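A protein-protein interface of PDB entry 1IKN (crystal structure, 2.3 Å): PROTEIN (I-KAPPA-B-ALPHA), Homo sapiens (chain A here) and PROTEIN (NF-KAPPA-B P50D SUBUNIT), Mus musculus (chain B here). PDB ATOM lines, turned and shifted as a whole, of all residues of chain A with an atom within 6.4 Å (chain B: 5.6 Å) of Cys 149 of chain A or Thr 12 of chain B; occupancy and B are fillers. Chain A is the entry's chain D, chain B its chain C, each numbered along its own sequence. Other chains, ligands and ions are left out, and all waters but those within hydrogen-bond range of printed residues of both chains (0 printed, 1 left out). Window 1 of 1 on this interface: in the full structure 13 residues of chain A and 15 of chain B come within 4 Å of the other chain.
Among the printed residues, pairs that only touch across the chains: Tyr 115 of chain A with Arg 11 of chain B (3.7 Å), Tyr 115 of chain A with Ala 13 of chain B (3.0 Å), Asn 116 of chain A with Arg 11 of chain B (3.7 Å), Pro 148 of chain A with Thr 12 of chain B (3.4 Å), Cys 149 of chain A with Arg 8 of chain B (3.3 Å), Cys 149 of chain A with Thr 12 of chain B (3.9 Å), Asn 150 of chain A with Arg 8 of chain B (3.6 Å) and Tyr 182 of chain A with Val 7 of chain B (2.9 Å).
Printed residues of chain A that touch a printed residue of chain B: Tyr 115, Asn 116, Pro 148, Cys 149, Asn 150, Arg 152 and Tyr 182. Hydrophobic or aromatic side chains of chain A within 4 Å of the printed part of chain B: Tyr 115, Pro 148 and Tyr 182. Of the 11 printed residues of chain B, 6 touch a printed residue of chain A. Among the printed residues, 11 pairs touch across the chains. Among the printed residues, no Asp or Glu carboxylate lies within 4 Å of a Lys or Arg side-chain nitrogen of the other chain.
Cys 149 of chain A touches three residues of chain B. Thr 12 of chain B touches just these residues of chain A: Pro 148 and Cys 149. Of the printed residues of chain A, Val 7 of chain B touches Asn 150 and Tyr 182. Printed residues of chain B within 4 Å of Arg 152 of chain A: Arg 8. Of the printed residues of chain A, Arg 11 of chain B touches Tyr 115 (3.7 Å) and Asn 116 (3.7 Å). Of the printed residues of chain B, Asn 116 of chain A touches Arg 11. Printed residues of chain B within 4 Å of Tyr 115 of chain A: Arg 11 (3.7 Å) and Ala 13 (3.0 Å). Pro 100 of chain B touches none of the printed residues of chain A. Leu 102 of chain B touches none of the printed residues of chain A. The nearest residue of chain B that does not touch Cys 149 of chain A is Val 7 of chain B (4.1 Å). The nearest residue of chain A that does not touch Thr 12 of chain B is Asn 116 of chain A (4.5 Å).
The guanidinium group of Arg 11 of chain B sits close to the backbone carbonyl oxygen of Ala 13 of chain B (3.3 Å). OE1 of Glu 147 of chain A lies within hydrogen-bond range of N of Cys 149 of chain A (3.1 Å). The backbone NH (N) of Arg 152 of chain A sits at hydrogen-bond distance from the side-chain carboxylate (OE2) of Glu 147 of chain A (2.8 Å). The side-chain hydroxyl (OH) of Tyr 182 of chain A sits close to the backbone carbonyl oxygen (O) of Pro 148 of chain A, at 3.3 Å. The side-chain amide nitrogen (ND2) of Asn 150 of chain A lies close to the guanidinium group (NE) of Arg 152 of chain A, 2.8 Å away. The backbone carbonyl oxygen (O) of Asn 150 of chain A lies within hydrogen-bond range of the backbone NH (N) of Tyr 182 of chain A.
The backbone carbonyl oxygen (O) of Val 7 of chain B sits close to the side-chain amide oxygen (OD1) of Asn 150 of chain A. N of Met 9 of chain B sits at hydrogen-bond distance from O of Cys 149 of chain A. The guanidinium group of Arg 8 of chain B lies close to the guanidinium group of Arg 152 of chain A.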
ATOM      1  N   TYR A 115      -7.006  -9.493  15.286  1.00  0.00           N
ATOM      2  CA  TYR A 115      -6.841 -10.933  15.068  1.00  0.00           C
ATOM      3  C   TYR A 115      -6.786 -11.324  13.609  1.00  0.00           C
ATOM      4  O   TYR A 115      -6.719 -12.500  13.283  1.00  0.00           O
ATOM      5  CB  TYR A 115      -7.959 -11.719  15.770  1.00  0.00           C
ATOM      6  CG  TYR A 115      -7.925 -11.586  17.275  1.00  0.00           C
ATOM      7  CD1 TYR A 115      -6.826 -11.014  17.920  1.00  0.00           C
ATOM      8  CD2 TYR A 115      -9.005 -11.997  18.053  1.00  0.00           C
ATOM      9  CE1 TYR A 115      -6.809 -10.845  19.299  1.00  0.00           C
ATOM     10  CE2 TYR A 115      -8.995 -11.833  19.434  1.00  0.00           C
ATOM     11  CZ  TYR A 115      -7.897 -11.252  20.046  1.00  0.00           C
ATOM     12  OH  TYR A 115      -7.909 -11.046  21.407  1.00  0.00           O
ATOM     13  N   ASN A 116      -6.826 -10.342  12.725  1.00  0.00           N
ATOM     14  CA  ASN A 116      -6.748 -10.632  11.305  1.00  0.00           C
ATOM     15  C   ASN A 116      -5.440 -10.079  10.778  1.00  0.00           C
ATOM     16  O   ASN A 116      -5.161 -10.137   9.590  1.00  0.00           O
ATOM     17  CB  ASN A 116      -7.943 -10.032  10.558  1.00  0.00           C
ATOM     18  CG  ASN A 116      -9.242 -10.745  10.884  1.00  0.00           C
ATOM     19  OD1 ASN A 116     -10.268 -10.542  10.228  1.00  0.00           O
ATOM     20  ND2 ASN A 116      -9.202 -11.590  11.909  1.00  0.00           N
ATOM     21  N   GLY A 117      -4.625  -9.564  11.695  1.00  0.00           N
ATOM     22  CA  GLY A 117      -3.340  -9.016  11.315  1.00  0.00           C
ATOM     23  C   GLY A 117      -3.475  -7.698  10.574  1.00  0.00           C
ATOM     24  O   GLY A 117      -2.528  -7.264   9.909  1.00  0.00           O
ATOM     25  N   GLU A 147       0.100  -7.686   5.845  1.00  0.00           N
ATOM     26  CA  GLU A 147      -0.915  -8.420   6.581  1.00  0.00           C
ATOM     27  C   GLU A 147      -0.516  -9.889   6.429  1.00  0.00           C
ATOM     28  O   GLU A 147      -0.084 -10.315   5.347  1.00  0.00           O
ATOM     29  CB  GLU A 147      -2.319  -8.102   6.026  1.00  0.00           C
ATOM     30  CG  GLU A 147      -2.564  -8.403   4.555  1.00  0.00           C
ATOM     31  CD  GLU A 147      -2.757  -9.870   4.286  1.00  0.00           C
ATOM     32  OE1 GLU A 147      -3.512 -10.523   5.038  1.00  0.00           O
ATOM     33  OE2 GLU A 147      -2.167 -10.371   3.314  1.00  0.00           O
ATOM     34  N   PRO A 148      -0.620 -10.671   7.520  1.00  0.00           N
ATOM     35  CA  PRO A 148      -0.279 -12.100   7.645  1.00  0.00           C
ATOM     36  C   PRO A 148      -0.880 -13.213   6.779  1.00  0.00           C
ATOM     37  O   PRO A 148      -0.234 -14.236   6.590  1.00  0.00           O
ATOM     38  CB  PRO A 148      -0.500 -12.376   9.139  1.00  0.00           C
ATOM     39  CG  PRO A 148      -1.584 -11.438   9.506  1.00  0.00           C
ATOM     40  CD  PRO A 148      -1.141 -10.164   8.804  1.00  0.00           C
ATOM     41  N   CYS A 149      -2.092 -13.041   6.263  1.00  0.00           N
ATOM     42  CA  CYS A 149      -2.711 -14.100   5.461  1.00  0.00           C
ATOM     43  C   CYS A 149      -1.953 -14.407   4.193  1.00  0.00           C
ATOM     44  O   CYS A 149      -1.672 -15.565   3.884  1.00  0.00           O
ATOM     45  CB  CYS A 149      -4.141 -13.719   5.071  1.00  0.00           C
ATOM     46  SG  CYS A 149      -5.297 -13.650   6.437  1.00  0.00           S
ATOM     47  N   ASN A 150      -1.639 -13.353   3.453  1.00  0.00           N
ATOM     48  CA  ASN A 150      -0.952 -13.474   2.182  1.00  0.00           C
ATOM     49  C   ASN A 150       0.204 -12.467   2.060  1.00  0.00           C
ATOM     50  O   ASN A 150       0.858 -12.412   1.028  1.00  0.00           O
ATOM     51  CB  ASN A 150      -1.984 -13.253   1.086  1.00  0.00           C
ATOM     52  CG  ASN A 150      -1.466 -13.587  -0.291  1.00  0.00           C
ATOM     53  OD1 ASN A 150      -0.734 -14.550  -0.464  1.00  0.00           O
ATOM     54  ND2 ASN A 150      -1.884 -12.799  -1.296  1.00  0.00           N
ATOM     55  N   GLY A 151       0.433 -11.664   3.105  1.00  0.00           N
ATOM     56  CA  GLY A 151       1.517 -10.691   3.093  1.00  0.00           C
ATOM     57  C   GLY A 151       1.264  -9.440   2.268  1.00  0.00           C
ATOM     58  O   GLY A 151       2.197  -8.711   1.905  1.00  0.00           O
ATOM     59  N   ARG A 152      -0.006  -9.177   1.982  1.00  0.00           N
ATOM     60  CA  ARG A 152      -0.378  -8.026   1.196  1.00  0.00           C
ATOM     61  C   ARG A 152      -0.163  -6.718   1.939  1.00  0.00           C
ATOM     62  O   ARG A 152      -0.315  -6.658   3.155  1.00  0.00           O
ATOM     63  CB  ARG A 152      -1.849  -8.166   0.737  1.00  0.00           C
ATOM     64  CG  ARG A 152      -2.031  -9.242  -0.356  1.00  0.00           C
ATOM     65  CD  ARG A 152      -3.470  -9.521  -0.819  1.00  0.00           C
ATOM     66  NE  ARG A 152      -3.421 -10.563  -1.853  1.00  0.00           N
ATOM     67  CZ  ARG A 152      -4.330 -10.770  -2.806  1.00  0.00           C
ATOM     68  NH1 ARG A 152      -5.410 -10.013  -2.890  1.00  0.00           N
ATOM     69  NH2 ARG A 152      -4.132 -11.712  -3.719  1.00  0.00           N
ATOM     70  N   TYR A 182       3.399 -13.471  -0.204  1.00  0.00           N
ATOM     71  CA  TYR A 182       3.993 -14.791   0.059  1.00  0.00           C
ATOM     72  C   TYR A 182       3.995 -15.601  -1.244  1.00  0.00           C
ATOM     73  O   TYR A 182       4.715 -16.574  -1.374  1.00  0.00           O
ATOM     74  CB  TYR A 182       3.201 -15.555   1.123  1.00  0.00           C
ATOM     75  CG  TYR A 182       3.099 -14.864   2.469  1.00  0.00           C
ATOM     76  CD1 TYR A 182       3.992 -13.855   2.839  1.00  0.00           C
ATOM     77  CD2 TYR A 182       2.108 -15.210   3.363  1.00  0.00           C
ATOM     78  CE1 TYR A 182       3.882 -13.218   4.044  1.00  0.00           C
ATOM     79  CE2 TYR A 182       2.001 -14.579   4.585  1.00  0.00           C
ATOM     80  CZ  TYR A 182       2.884 -13.585   4.918  1.00  0.00           C
ATOM     81  OH  TYR A 182       2.740 -12.948   6.139  1.00  0.00           O
ATOM     82  N   VAL B   7       2.195 -20.391   1.456  1.00  0.00           N
ATOM     83  CA  VAL B   7       1.775 -19.344   0.530  1.00  0.00           C
ATOM     84  C   VAL B   7       0.653 -18.429   1.040  1.00  0.00           C
ATOM     85  O   VAL B   7       0.779 -17.201   1.033  1.00  0.00           O
ATOM     86  CB  VAL B   7       1.378 -20.022  -0.812  1.00  0.00           C
ATOM     87  CG1 VAL B   7       0.257 -19.287  -1.496  1.00  0.00           C
ATOM     88  CG2 VAL B   7       2.598 -20.114  -1.699  1.00  0.00           C
ATOM     89  N   ARG B   8      -0.456 -19.014   1.457  1.00  0.00           N
ATOM     90  CA  ARG B   8      -1.549 -18.213   1.976  1.00  0.00           C
ATOM     91  C   ARG B   8      -2.344 -19.004   2.994  1.00  0.00           C
ATOM     92  O   ARG B   8      -2.526 -20.205   2.834  1.00  0.00           O
ATOM     93  CB  ARG B   8      -2.454 -17.717   0.833  1.00  0.00           C
ATOM     94  CG  ARG B   8      -3.839 -17.258   1.291  1.00  0.00           C
ATOM     95  CD  ARG B   8      -4.345 -15.934   0.664  1.00  0.00           C
ATOM     96  NE  ARG B   8      -4.250 -15.879  -0.794  1.00  0.00           N
ATOM     97  CZ  ARG B   8      -4.837 -14.950  -1.553  1.00  0.00           C
ATOM     98  NH1 ARG B   8      -5.595 -14.012  -1.005  1.00  0.00           N
ATOM     99  NH2 ARG B   8      -4.683 -14.972  -2.872  1.00  0.00           N
ATOM    100  N   MET B   9      -2.785 -18.320   4.046  1.00  0.00           N
ATOM    101  CA  MET B   9      -3.589 -18.918   5.114  1.00  0.00           C
ATOM    102  C   MET B   9      -4.869 -18.099   5.289  1.00  0.00           C
ATOM    103  O   MET B   9      -4.803 -16.884   5.397  1.00  0.00           O
ATOM    104  CB  MET B   9      -2.818 -18.906   6.429  1.00  0.00           C
ATOM    105  CG  MET B   9      -1.637 -19.856   6.485  1.00  0.00           C
ATOM    106  SD  MET B   9      -0.902 -19.833   8.133  1.00  0.00           S
ATOM    107  CE  MET B   9      -2.313 -20.471   9.121  1.00  0.00           C
ATOM    108  N   ASP B  10      -6.030 -18.750   5.341  1.00  0.00           N
ATOM    109  CA  ASP B  10      -7.269 -18.007   5.481  1.00  0.00           C
ATOM    110  C   ASP B  10      -7.442 -17.385   6.860  1.00  0.00           C
ATOM    111  O   ASP B  10      -8.290 -16.525   7.049  1.00  0.00           O
ATOM    112  CB  ASP B  10      -8.478 -18.875   5.114  1.00  0.00           C
ATOM    113  CG  ASP B  10      -8.762 -19.968   6.130  1.00  0.00           C
ATOM    114  OD1 ASP B  10      -8.012 -20.117   7.124  1.00  0.00           O
ATOM    115  OD2 ASP B  10      -9.754 -20.697   5.923  1.00  0.00           O
ATOM    116  N   ARG B  11      -6.624 -17.810   7.819  1.00  0.00           N
ATOM    117  CA  ARG B  11      -6.678 -17.279   9.172  1.00  0.00           C
ATOM    118  C   ARG B  11      -5.294 -17.423   9.777  1.00  0.00           C
ATOM    119  O   ARG B  11      -4.632 -18.439   9.576  1.00  0.00           O
ATOM    120  CB  ARG B  11      -7.684 -18.058  10.025  1.00  0.00           C
ATOM    121  CG  ARG B  11      -8.072 -17.351  11.330  1.00  0.00           C
ATOM    122  CD  ARG B  11      -9.159 -16.292  11.090  1.00  0.00           C
ATOM    123  NE  ARG B  11      -9.246 -15.301  12.167  1.00  0.00           N
ATOM    124  CZ  ARG B  11      -9.697 -15.541  13.397  1.00  0.00           C
ATOM    125  NH1 ARG B  11     -10.119 -16.754  13.734  1.00  0.00           N
ATOM    126  NH2 ARG B  11      -9.720 -14.562  14.298  1.00  0.00           N
ATOM    127  N   THR B  12      -4.855 -16.411  10.516  1.00  0.00           N
ATOM    128  CA  THR B  12      -3.546 -16.428  11.150  1.00  0.00           C
ATOM    129  C   THR B  12      -3.692 -16.203  12.645  1.00  0.00           C
ATOM    130  O   THR B  12      -2.726 -15.840  13.321  1.00  0.00           O
ATOM    131  CB  THR B  12      -2.643 -15.331  10.583  1.00  0.00           C
ATOM    132  OG1 THR B  12      -3.310 -14.067  10.685  1.00  0.00           O
ATOM    133  CG2 THR B  12      -2.335 -15.598   9.131  1.00  0.00           C
ATOM    134  N   ALA B  13      -4.908 -16.395  13.152  1.00  0.00           N
ATOM    135  CA  ALA B  13      -5.197 -16.257  14.576  1.00  0.00           C
ATOM    136  C   ALA B  13      -6.217 -17.316  14.950  1.00  0.00           C
ATOM    137  O   ALA B  13      -6.957 -17.796  14.092  1.00  0.00           O
ATOM    138  CB  ALA B  13      -5.756 -14.900  14.882  1.00  0.00           C
ATOM    139  N   GLY B  14      -6.259 -17.669  16.234  1.00  0.00           N
ATOM    140  CA  GLY B  14      -7.202 -18.665  16.691  1.00  0.00           C
ATOM    141  C   GLY B  14      -7.319 -18.735  18.194  1.00  0.00           C
ATOM    142  O   GLY B  14      -6.476 -18.211  18.930  1.00  0.00           O
ATOM    143  N   PRO B 100       4.338 -16.550  12.100  1.00  0.00           N
ATOM    144  CA  PRO B 100       3.588 -16.072  13.274  1.00  0.00           C
ATOM    145  C   PRO B 100       2.099 -16.415  13.239  1.00  0.00           C
ATOM    146  O   PRO B 100       1.447 -16.294  12.213  1.00  0.00           O
ATOM    147  CB  PRO B 100       3.834 -14.570  13.249  1.00  0.00           C
ATOM    148  CG  PRO B 100       5.212 -14.468  12.660  1.00  0.00           C
ATOM    149  CD  PRO B 100       5.160 -15.465  11.527  1.00  0.00           C
ATOM    150  N   PHE B 101       1.583 -16.860  14.379  1.00  0.00           N
ATOM    151  CA  PHE B 101       0.185 -17.246  14.539  1.00  0.00           C
ATOM    152  C   PHE B 101      -0.211 -16.746  15.918  1.00  0.00           C
ATOM    153  O   PHE B 101       0.582 -16.856  16.861  1.00  0.00           O
ATOM    154  CB  PHE B 101       0.035 -18.774  14.466  1.00  0.00           C
ATOM    155  CG  PHE B 101      -1.384 -19.259  14.629  1.00  0.00           C
ATOM    156  CD1 PHE B 101      -1.925 -19.476  15.895  1.00  0.00           C
ATOM    157  CD2 PHE B 101      -2.178 -19.517  13.507  1.00  0.00           C
ATOM    158  CE1 PHE B 101      -3.248 -19.954  16.043  1.00  0.00           C
ATOM    159  CE2 PHE B 101      -3.495 -19.990  13.633  1.00  0.00           C
ATOM    160  CZ  PHE B 101      -4.035 -20.213  14.899  1.00  0.00           C
ATOM    161  N   LEU B 102      -1.422 -16.205  16.046  1.00  0.00           N
ATOM    162  CA  LEU B 102      -1.850 -15.672  17.335  1.00  0.00           C
ATOM    163  C   LEU B 102      -2.971 -16.476  17.989  1.00  0.00           C
ATOM    164  O   LEU B 102      -4.055 -16.629  17.417  1.00  0.00           O
ATOM    165  CB  LEU B 102      -2.288 -14.216  17.158  1.00  0.00           C
ATOM    166  CG  LEU B 102      -2.413 -13.225  18.330  1.00  0.00           C
ATOM    167  CD1 LEU B 102      -3.558 -13.636  19.228  1.00  0.00           C
ATOM    168  CD2 LEU B 102      -1.099 -13.135  19.106  1.00  0.00           C
